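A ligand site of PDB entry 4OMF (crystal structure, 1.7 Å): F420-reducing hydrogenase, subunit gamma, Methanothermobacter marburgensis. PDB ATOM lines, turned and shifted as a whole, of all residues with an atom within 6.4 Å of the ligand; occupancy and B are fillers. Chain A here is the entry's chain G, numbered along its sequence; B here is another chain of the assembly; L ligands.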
ATOM      1  N   SER A  55      26.015 -26.939 -23.012  1.00  0.00           N
ATOM      2  CA  SER A  55      24.927 -27.536 -22.211  1.00  0.00           C
ATOM      3  C   SER A  55      25.234 -27.350 -20.728  1.00  0.00           C
ATOM      4  O   SER A  55      25.520 -28.309 -19.995  1.00  0.00           O
ATOM      5  CB  SER A  55      24.721 -29.010 -22.571  1.00  0.00           C
ATOM      6  OG  SER A  55      24.209 -29.131 -23.898  1.00  0.00           O
ATOM      7  N   GLY A  56      25.165 -26.076 -20.308  1.00  0.00           N
ATOM      8  CA  GLY A  56      25.397 -25.682 -18.938  1.00  0.00           C
ATOM      9  C   GLY A  56      24.087 -25.211 -18.360  1.00  0.00           C
ATOM     10  O   GLY A  56      23.051 -25.448 -18.953  1.00  0.00           O
ATOM     11  N   CYS A  57      24.129 -24.591 -17.180  1.00  0.00           N
ATOM     12  CA  CYS A  57      22.917 -24.093 -16.541  1.00  0.00           C
ATOM     13  C   CYS A  57      23.033 -22.595 -16.238  1.00  0.00           C
ATOM     14  O   CYS A  57      22.127 -21.988 -15.664  1.00  0.00           O
ATOM     15  CB  CYS A  57      22.608 -24.874 -15.258  1.00  0.00           C
ATOM     16  SG  CYS A  57      23.657 -24.255 -13.875  1.00  0.00           S
ATOM     17  N   THR A  58      24.173 -22.034 -16.662  1.00  0.00           N
ATOM     18  CA  THR A  58      24.539 -20.627 -16.490  1.00  0.00           C
ATOM     19  C   THR A  58      24.890 -20.282 -15.040  1.00  0.00           C
ATOM     20  O   THR A  58      25.198 -19.131 -14.710  1.00  0.00           O
ATOM     21  CB  THR A  58      23.427 -19.699 -17.089  1.00  0.00           C
ATOM     22  OG1 THR A  58      23.223 -20.084 -18.452  1.00  0.00           O
ATOM     23  CG2 THR A  58      23.837 -18.227 -17.094  1.00  0.00           C
ATOM     24  N   GLY A  59      24.880 -21.285 -14.161  1.00  0.00           N
ATOM     25  CA  GLY A  59      25.273 -21.040 -12.774  1.00  0.00           C
ATOM     26  C   GLY A  59      26.693 -20.531 -12.662  1.00  0.00           C
ATOM     27  O   GLY A  59      27.009 -19.771 -11.754  1.00  0.00           O
ATOM     28  N   ASP A  60      27.571 -20.938 -13.569  1.00  0.00           N
ATOM     29  CA  ASP A  60      28.959 -20.462 -13.491  1.00  0.00           C
ATOM     30  C   ASP A  60      29.079 -18.984 -13.800  1.00  0.00           C
ATOM     31  O   ASP A  60      29.805 -18.253 -13.097  1.00  0.00           O
ATOM     32  CB  ASP A  60      29.820 -21.270 -14.435  1.00  0.00           C
ATOM     33  CG  ASP A  60      29.586 -22.742 -14.242  1.00  0.00           C
ATOM     34  OD1 ASP A  60      30.171 -23.332 -13.342  1.00  0.00           O
ATOM     35  OD2 ASP A  60      28.727 -23.257 -14.944  1.00  0.00           O
ATOM     36  N   GLU A 102      31.283 -22.880 -20.593  1.00  0.00           N
ATOM     37  CA  GLU A 102      30.442 -23.457 -19.565  1.00  0.00           C
ATOM     38  C   GLU A 102      29.563 -24.577 -20.147  1.00  0.00           C
ATOM     39  O   GLU A 102      29.001 -24.419 -21.231  1.00  0.00           O
ATOM     40  CB  GLU A 102      29.593 -22.359 -18.949  1.00  0.00           C
ATOM     41  CG  GLU A 102      28.571 -22.918 -17.989  1.00  0.00           C
ATOM     42  CD  GLU A 102      27.439 -21.956 -17.837  1.00  0.00           C
ATOM     43  OE1 GLU A 102      27.673 -20.902 -17.217  1.00  0.00           O
ATOM     44  OE2 GLU A 102      26.345 -22.256 -18.366  1.00  0.00           O
ATOM     45  N   GLY A 103      29.436 -25.691 -19.408  1.00  0.00           N
ATOM     46  CA  GLY A 103      28.584 -26.778 -19.853  1.00  0.00           C
ATOM     47  C   GLY A 103      29.312 -27.905 -20.564  1.00  0.00           C
ATOM     48  O   GLY A 103      30.385 -27.714 -21.169  1.00  0.00           O
ATOM     49  N   SER A 104      28.720 -29.090 -20.494  1.00  0.00           N
ATOM     50  CA  SER A 104      29.187 -30.212 -21.306  1.00  0.00           C
ATOM     51  C   SER A 104      28.699 -30.006 -22.740  1.00  0.00           C
ATOM     52  O   SER A 104      27.954 -29.077 -23.025  1.00  0.00           O
ATOM     53  CB  SER A 104      28.679 -31.553 -20.722  1.00  0.00           C
ATOM     54  OG  SER A 104      27.270 -31.503 -20.525  1.00  0.00           O
ATOM     55  N   PHE A 129      34.909 -24.079 -17.731  1.00  0.00           N
ATOM     56  CA  PHE A 129      34.327 -23.199 -16.718  1.00  0.00           C
ATOM     57  C   PHE A 129      33.216 -23.931 -15.955  1.00  0.00           C
ATOM     58  O   PHE A 129      32.082 -24.026 -16.437  1.00  0.00           O
ATOM     59  CB  PHE A 129      33.791 -21.960 -17.451  1.00  0.00           C
ATOM     60  CG  PHE A 129      33.317 -20.843 -16.561  1.00  0.00           C
ATOM     61  CD1 PHE A 129      33.822 -20.650 -15.288  1.00  0.00           C
ATOM     62  CD2 PHE A 129      32.378 -19.950 -17.053  1.00  0.00           C
ATOM     63  CE1 PHE A 129      33.365 -19.573 -14.505  1.00  0.00           C
ATOM     64  CE2 PHE A 129      31.941 -18.869 -16.294  1.00  0.00           C
ATOM     65  CZ  PHE A 129      32.443 -18.688 -15.009  1.00  0.00           C
ATOM     66  N   GLY A 130      33.539 -24.507 -14.795  1.00  0.00           N
ATOM     67  CA  GLY A 130      32.566 -25.279 -14.051  1.00  0.00           C
ATOM     68  C   GLY A 130      32.682 -26.769 -14.365  1.00  0.00           C
ATOM     69  O   GLY A 130      33.195 -27.164 -15.399  1.00  0.00           O
ATOM     70  N   SER A 131      32.229 -27.616 -13.453  1.00  0.00           N
ATOM     71  CA  SER A 131      32.401 -29.055 -13.622  1.00  0.00           C
ATOM     72  C   SER A 131      31.629 -29.692 -14.793  1.00  0.00           C
ATOM     73  O   SER A 131      32.045 -30.744 -15.234  1.00  0.00           O
ATOM     74  CB  SER A 131      32.020 -29.796 -12.330  1.00  0.00           C
ATOM     75  OG  SER A 131      32.926 -29.503 -11.289  1.00  0.00           O
ATOM     76  N   CYS A 132      30.526 -29.113 -15.275  1.00  0.00           N
ATOM     77  CA  CYS A 132      29.899 -29.743 -16.446  1.00  0.00           C
ATOM     78  C   CYS A 132      30.866 -29.738 -17.636  1.00  0.00           C
ATOM     79  O   CYS A 132      31.020 -30.747 -18.318  1.00  0.00           O
ATOM     80  CB  CYS A 132      28.602 -29.053 -16.856  1.00  0.00           C
ATOM     81  SG  CYS A 132      27.217 -29.507 -15.770  1.00  0.00           S
ATOM     82  N   ALA A 133      31.519 -28.615 -17.860  1.00  0.00           N
ATOM     83  CA  ALA A 133      32.506 -28.522 -18.933  1.00  0.00           C
ATOM     84  C   ALA A 133      33.767 -29.310 -18.593  1.00  0.00           C
ATOM     85  O   ALA A 133      34.411 -29.893 -19.463  1.00  0.00           O
ATOM     86  CB  ALA A 133      32.854 -27.059 -19.194  1.00  0.00           C
ATOM     87  N   GLY A 136      31.925 -33.207 -16.879  1.00  0.00           N
ATOM     88  CA  GLY A 136      30.611 -33.708 -17.248  1.00  0.00           C
ATOM     89  C   GLY A 136      29.608 -33.461 -16.140  1.00  0.00           C
ATOM     90  O   GLY A 136      28.424 -33.220 -16.404  1.00  0.00           O
ATOM     91  N   CYS A 137      30.083 -33.486 -14.893  1.00  0.00           N
ATOM     92  CA  CYS A 137      29.248 -33.226 -13.713  1.00  0.00           C
ATOM     93  C   CYS A 137      27.945 -34.027 -13.809  1.00  0.00           C
ATOM     94  O   CYS A 137      27.983 -35.196 -14.186  1.00  0.00           O
ATOM     95  CB  CYS A 137      29.014 -31.709 -13.571  1.00  0.00           C
ATOM     96  SG  CYS A 137      28.349 -31.195 -11.948  1.00  0.00           S
ATOM     97  N   PHE A 138      26.795 -33.444 -13.442  1.00  0.00           N
ATOM     98  CA  PHE A 138      25.566 -34.255 -13.393  1.00  0.00           C
ATOM     99  C   PHE A 138      25.048 -34.671 -14.779  1.00  0.00           C
ATOM    100  O   PHE A 138      24.221 -35.564 -14.866  1.00  0.00           O
ATOM    101  CB  PHE A 138      24.449 -33.496 -12.640  1.00  0.00           C
ATOM    102  CG  PHE A 138      23.678 -32.568 -13.525  1.00  0.00           C
ATOM    103  CD1 PHE A 138      22.457 -32.976 -14.063  1.00  0.00           C
ATOM    104  CD2 PHE A 138      24.195 -31.345 -13.880  1.00  0.00           C
ATOM    105  CE1 PHE A 138      21.741 -32.117 -14.914  1.00  0.00           C
ATOM    106  CE2 PHE A 138      23.512 -30.489 -14.718  1.00  0.00           C
ATOM    107  CZ  PHE A 138      22.284 -30.869 -15.245  1.00  0.00           C
ATOM    108  N   THR A 139      25.534 -34.055 -15.862  1.00  0.00           N
ATOM    109  CA  THR A 139      25.096 -34.505 -17.188  1.00  0.00           C
ATOM    110  C   THR A 139      25.699 -35.886 -17.532  1.00  0.00           C
ATOM    111  O   THR A 139      25.257 -36.537 -18.465  1.00  0.00           O
ATOM    112  CB  THR A 139      25.420 -33.486 -18.281  1.00  0.00           C
ATOM    113  OG1 THR A 139      26.842 -33.408 -18.510  1.00  0.00           O
ATOM    114  CG2 THR A 139      24.912 -32.117 -17.832  1.00  0.00           C
ATOM    115  N   GLY A 170      33.860 -27.191 -10.044  1.00  0.00           N
ATOM    116  CA  GLY A 170      32.975 -26.581  -9.076  1.00  0.00           C
ATOM    117  C   GLY A 170      31.591 -26.515  -9.671  1.00  0.00           C
ATOM    118  O   GLY A 170      31.426 -26.361 -10.883  1.00  0.00           O
ATOM    119  N   CYS A 171      30.585 -26.578  -8.800  1.00  0.00           N
ATOM    120  CA  CYS A 171      29.220 -26.575  -9.286  1.00  0.00           C
ATOM    121  C   CYS A 171      28.323 -25.587  -8.525  1.00  0.00           C
ATOM    122  O   CYS A 171      27.521 -25.982  -7.695  1.00  0.00           O
ATOM    123  CB  CYS A 171      28.663 -27.988  -9.203  1.00  0.00           C
ATOM    124  SG  CYS A 171      27.075 -28.074 -10.035  1.00  0.00           S
ATOM    125  N   PRO A 172      28.507 -24.287  -8.769  1.00  0.00           N
ATOM    126  CA  PRO A 172      29.528 -23.666  -9.630  1.00  0.00           C
ATOM    127  C   PRO A 172      30.821 -23.407  -8.865  1.00  0.00           C
ATOM    128  O   PRO A 172      30.830 -23.441  -7.630  1.00  0.00           O
ATOM    129  CB  PRO A 172      28.879 -22.328 -10.029  1.00  0.00           C
ATOM    130  CG  PRO A 172      28.102 -21.951  -8.778  1.00  0.00           C
ATOM    131  CD  PRO A 172      27.629 -23.273  -8.140  1.00  0.00           C
ATOM    132  N   PRO A 173      31.908 -23.100  -9.590  1.00  0.00           N
ATOM    133  CA  PRO A 173      33.096 -22.586  -8.920  1.00  0.00           C
ATOM    134  C   PRO A 173      32.729 -21.338  -8.137  1.00  0.00           C
ATOM    135  O   PRO A 173      31.839 -20.565  -8.540  1.00  0.00           O
ATOM    136  CB  PRO A 173      34.064 -22.268 -10.093  1.00  0.00           C
ATOM    137  CG  PRO A 173      33.506 -23.027 -11.290  1.00  0.00           C
ATOM    138  CD  PRO A 173      32.029 -23.082 -11.067  1.00  0.00           C
ATOM    139  N   ILE A 250      27.059 -35.480  -7.745  1.00  0.00           N
ATOM    140  CA  ILE A 250      26.895 -34.906  -9.066  1.00  0.00           C
ATOM    141  C   ILE A 250      28.177 -35.070  -9.904  1.00  0.00           C
ATOM    142  O   ILE A 250      28.279 -34.507 -10.992  1.00  0.00           O
ATOM    143  CB  ILE A 250      26.517 -33.416  -8.978  1.00  0.00           C
ATOM    144  CG1 ILE A 250      27.516 -32.681  -8.067  1.00  0.00           C
ATOM    145  CG2 ILE A 250      25.087 -33.298  -8.405  1.00  0.00           C
ATOM    146  CD1 ILE A 250      27.486 -31.151  -8.212  1.00  0.00           C
ATOM    147  N   ARG B  41      19.211 -31.880 -22.044  1.00  0.00           N
ATOM    148  CA  ARG B  41      19.936 -32.641 -21.018  1.00  0.00           C
ATOM    149  C   ARG B  41      19.039 -33.760 -20.437  1.00  0.00           C
ATOM    150  O   ARG B  41      19.523 -34.822 -20.074  1.00  0.00           O
ATOM    151  CB  ARG B  41      20.455 -31.676 -19.934  1.00  0.00           C
ATOM    152  CG  ARG B  41      21.610 -30.820 -20.503  1.00  0.00           C
ATOM    153  CD  ARG B  41      21.991 -29.604 -19.690  1.00  0.00           C
ATOM    154  NE  ARG B  41      20.787 -28.823 -19.441  1.00  0.00           N
ATOM    155  CZ  ARG B  41      20.525 -28.166 -18.314  1.00  0.00           C
ATOM    156  NH1 ARG B  41      21.401 -28.112 -17.303  1.00  0.00           N
ATOM    157  NH2 ARG B  41      19.369 -27.540 -18.218  1.00  0.00           N
ATOM    158  N   ARG B  61      19.632 -28.324 -11.028  1.00  0.00           N
ATOM    159  CA  ARG B  61      20.671 -28.007 -12.003  1.00  0.00           C
ATOM    160  C   ARG B  61      20.119 -27.855 -13.416  1.00  0.00           C
ATOM    161  O   ARG B  61      20.859 -27.698 -14.378  1.00  0.00           O
ATOM    162  CB  ARG B  61      21.793 -29.047 -11.967  1.00  0.00           C
ATOM    163  CG  ARG B  61      22.650 -28.871 -10.694  1.00  0.00           C
ATOM    164  CD  ARG B  61      23.535 -30.084 -10.283  1.00  0.00           C
ATOM    165  NE  ARG B  61      24.422 -29.588  -9.235  1.00  0.00           N
ATOM    166  CZ  ARG B  61      24.081 -29.365  -7.974  1.00  0.00           C
ATOM    167  NH1 ARG B  61      22.879 -29.711  -7.498  1.00  0.00           N
ATOM    168  NH2 ARG B  61      24.973 -28.782  -7.157  1.00  0.00           N
ATOM    169  N   CYS B  63      18.862 -25.161 -14.004  1.00  0.00           N
ATOM    170  CA  CYS B  63      19.193 -23.753 -14.191  1.00  0.00           C
ATOM    171  C   CYS B  63      19.882 -23.119 -13.001  1.00  0.00           C
ATOM    172  O   CYS B  63      19.392 -23.226 -11.855  1.00  0.00           O
ATOM    173  CB  CYS B  63      17.922 -22.947 -14.471  1.00  0.00           C
ATOM    174  SG  CYS B  63      18.356 -21.228 -14.848  1.00  0.00           S
ATOM    175  N   GLY B  64      21.001 -22.425 -13.270  1.00  0.00           N
ATOM    176  CA  GLY B  64      21.777 -21.798 -12.203  1.00  0.00           C
ATOM    177  C   GLY B  64      21.420 -20.339 -11.963  1.00  0.00           C
ATOM    178  O   GLY B  64      21.995 -19.680 -11.084  1.00  0.00           O
ATOM    179  N   ILE B 149      23.686 -20.655  -5.025  1.00  0.00           N
ATOM    180  CA  ILE B 149      23.359 -21.279  -6.305  1.00  0.00           C
ATOM    181  C   ILE B 149      23.354 -22.800  -6.047  1.00  0.00           C
ATOM    182  O   ILE B 149      24.287 -23.317  -5.446  1.00  0.00           O
ATOM    183  CB  ILE B 149      24.390 -20.905  -7.410  1.00  0.00           C
ATOM    184  CG1 ILE B 149      24.336 -19.396  -7.703  1.00  0.00           C
ATOM    185  CG2 ILE B 149      24.097 -21.694  -8.686  1.00  0.00           C
ATOM    186  CD1 ILE B 149      25.606 -18.787  -8.429  1.00  0.00           C
ATOM    187  N   HIS B 150      22.293 -23.496  -6.486  1.00  0.00           N
ATOM    188  CA  HIS B 150      22.045 -24.913  -6.160  1.00  0.00           C
ATOM    189  C   HIS B 150      22.070 -25.155  -4.647  1.00  0.00           C
ATOM    190  O   HIS B 150      22.949 -25.850  -4.121  1.00  0.00           O
ATOM    191  CB  HIS B 150      23.051 -25.814  -6.904  1.00  0.00           C
ATOM    192  CG  HIS B 150      23.076 -25.561  -8.375  1.00  0.00           C
ATOM    193  ND1 HIS B 150      21.927 -25.262  -9.084  1.00  0.00           N
ATOM    194  CD2 HIS B 150      24.098 -25.516  -9.261  1.00  0.00           C
ATOM    195  CE1 HIS B 150      22.243 -25.047 -10.344  1.00  0.00           C
ATOM    196  NE2 HIS B 150      23.556 -25.208 -10.487  1.00  0.00           N
HETATM  197 FE1  LIG L   1      25.518 -25.564 -13.792  1.00  0.00          FE
HETATM  198 FE2  LIG L   1      27.110 -27.530 -14.529  1.00  0.00          FE
HETATM  199 FE3  LIG L   1      27.027 -26.798 -11.965  1.00  0.00          FE
HETATM  200 FE4  LIG L   1      28.082 -25.036 -13.790  1.00  0.00          FE
HETATM  201  S1  LIG L   1      28.960 -27.069 -13.205  1.00  0.00           S
HETATM  202  S2  LIG L   1      26.648 -24.538 -12.057  1.00  0.00           S
HETATM  203  S3  LIG L   1      26.856 -25.591 -15.679  1.00  0.00           S
HETATM  204  S4  LIG L   1      25.276 -27.729 -13.150  1.00  0.00           S
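N of Ser 131 sits close to S1 of the ligand (3.3 Å). FE1 of the ligand is bound by SG of Cys 57, 2.3 Å away. The side-chain sulfur (SG) of Cys 132 is bound to an iron atom (FE2) of the ligand (2.3 Å). S3 of the ligand sits close to N of Cys 57 (3.3 Å). A sulfur (S1) of the ligand sits close to the backbone NH (N) of Cys 132. SG of Cys 171 is bound to FE3 of the ligand, at 2.3 Å. The side-chain carboxylate (OD2) of Asp 60 is bound to an iron atom (FE4) of the ligand. A ring nitrogen (NE2) of His 150 of chain B sits close to a sulfur (S2) of the ligand, 3.5 Å away.
O of Ser 131 lies within hydrogen-bond range of N of Cys 137 (3.4 Å). O of Ser 131 is in hydrogen-bond range of N of Gly 136, at 3.0 Å. N of Gly 170 is in hydrogen-bond range of OG of Ser 131 (2.8 Å). OE2 of Glu 102 is in hydrogen-bond range of N of Cys 57, 3.4 Å away. OE2 of Glu 102 lies within hydrogen-bond range of N of Thr 58, at 2.8 Å. The backbone NH (N) of Phe 138 is in hydrogen-bond range of the backbone carbonyl oxygen (O) of Ile 250 (3.1 Å). The side-chain sulfur (SG) of Cys 57 lies close to the backbone NH (N) of Gly 59 (3.2 Å). The guanidinium group (NE) of Arg 61 of chain B lies close to the side-chain sulfur (SG) of Cys 171.
A sulfur (S1) of the ligand lies close to the backbone carbonyl oxygen of Gly 170, 3.5 Å away. N of Pro 172 sits close to S2 of the ligand. Gly 56 touches the ligand. Gly 59 touches the ligand (CA to S2, 3.8 Å). CG of Glu 102 touches S3 of the ligand, 3.9 Å away. C of Gly 130 touches S1 of the ligand (3.9 Å). Phe 138 touches the ligand (CE2 to S4, 3.6 Å). CG of Arg 61 of chain B touches S4 of the ligand, at 3.8 Å. Hydrophobic or aromatic side chains that line the ligand: Phe 138, Pro 172 and His 150 of chain B. Of the 29 residues printed, 14 come within 4 Å of the ligand. Along chain A the residues within 4 Å of the ligand span positions 56 to 172.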
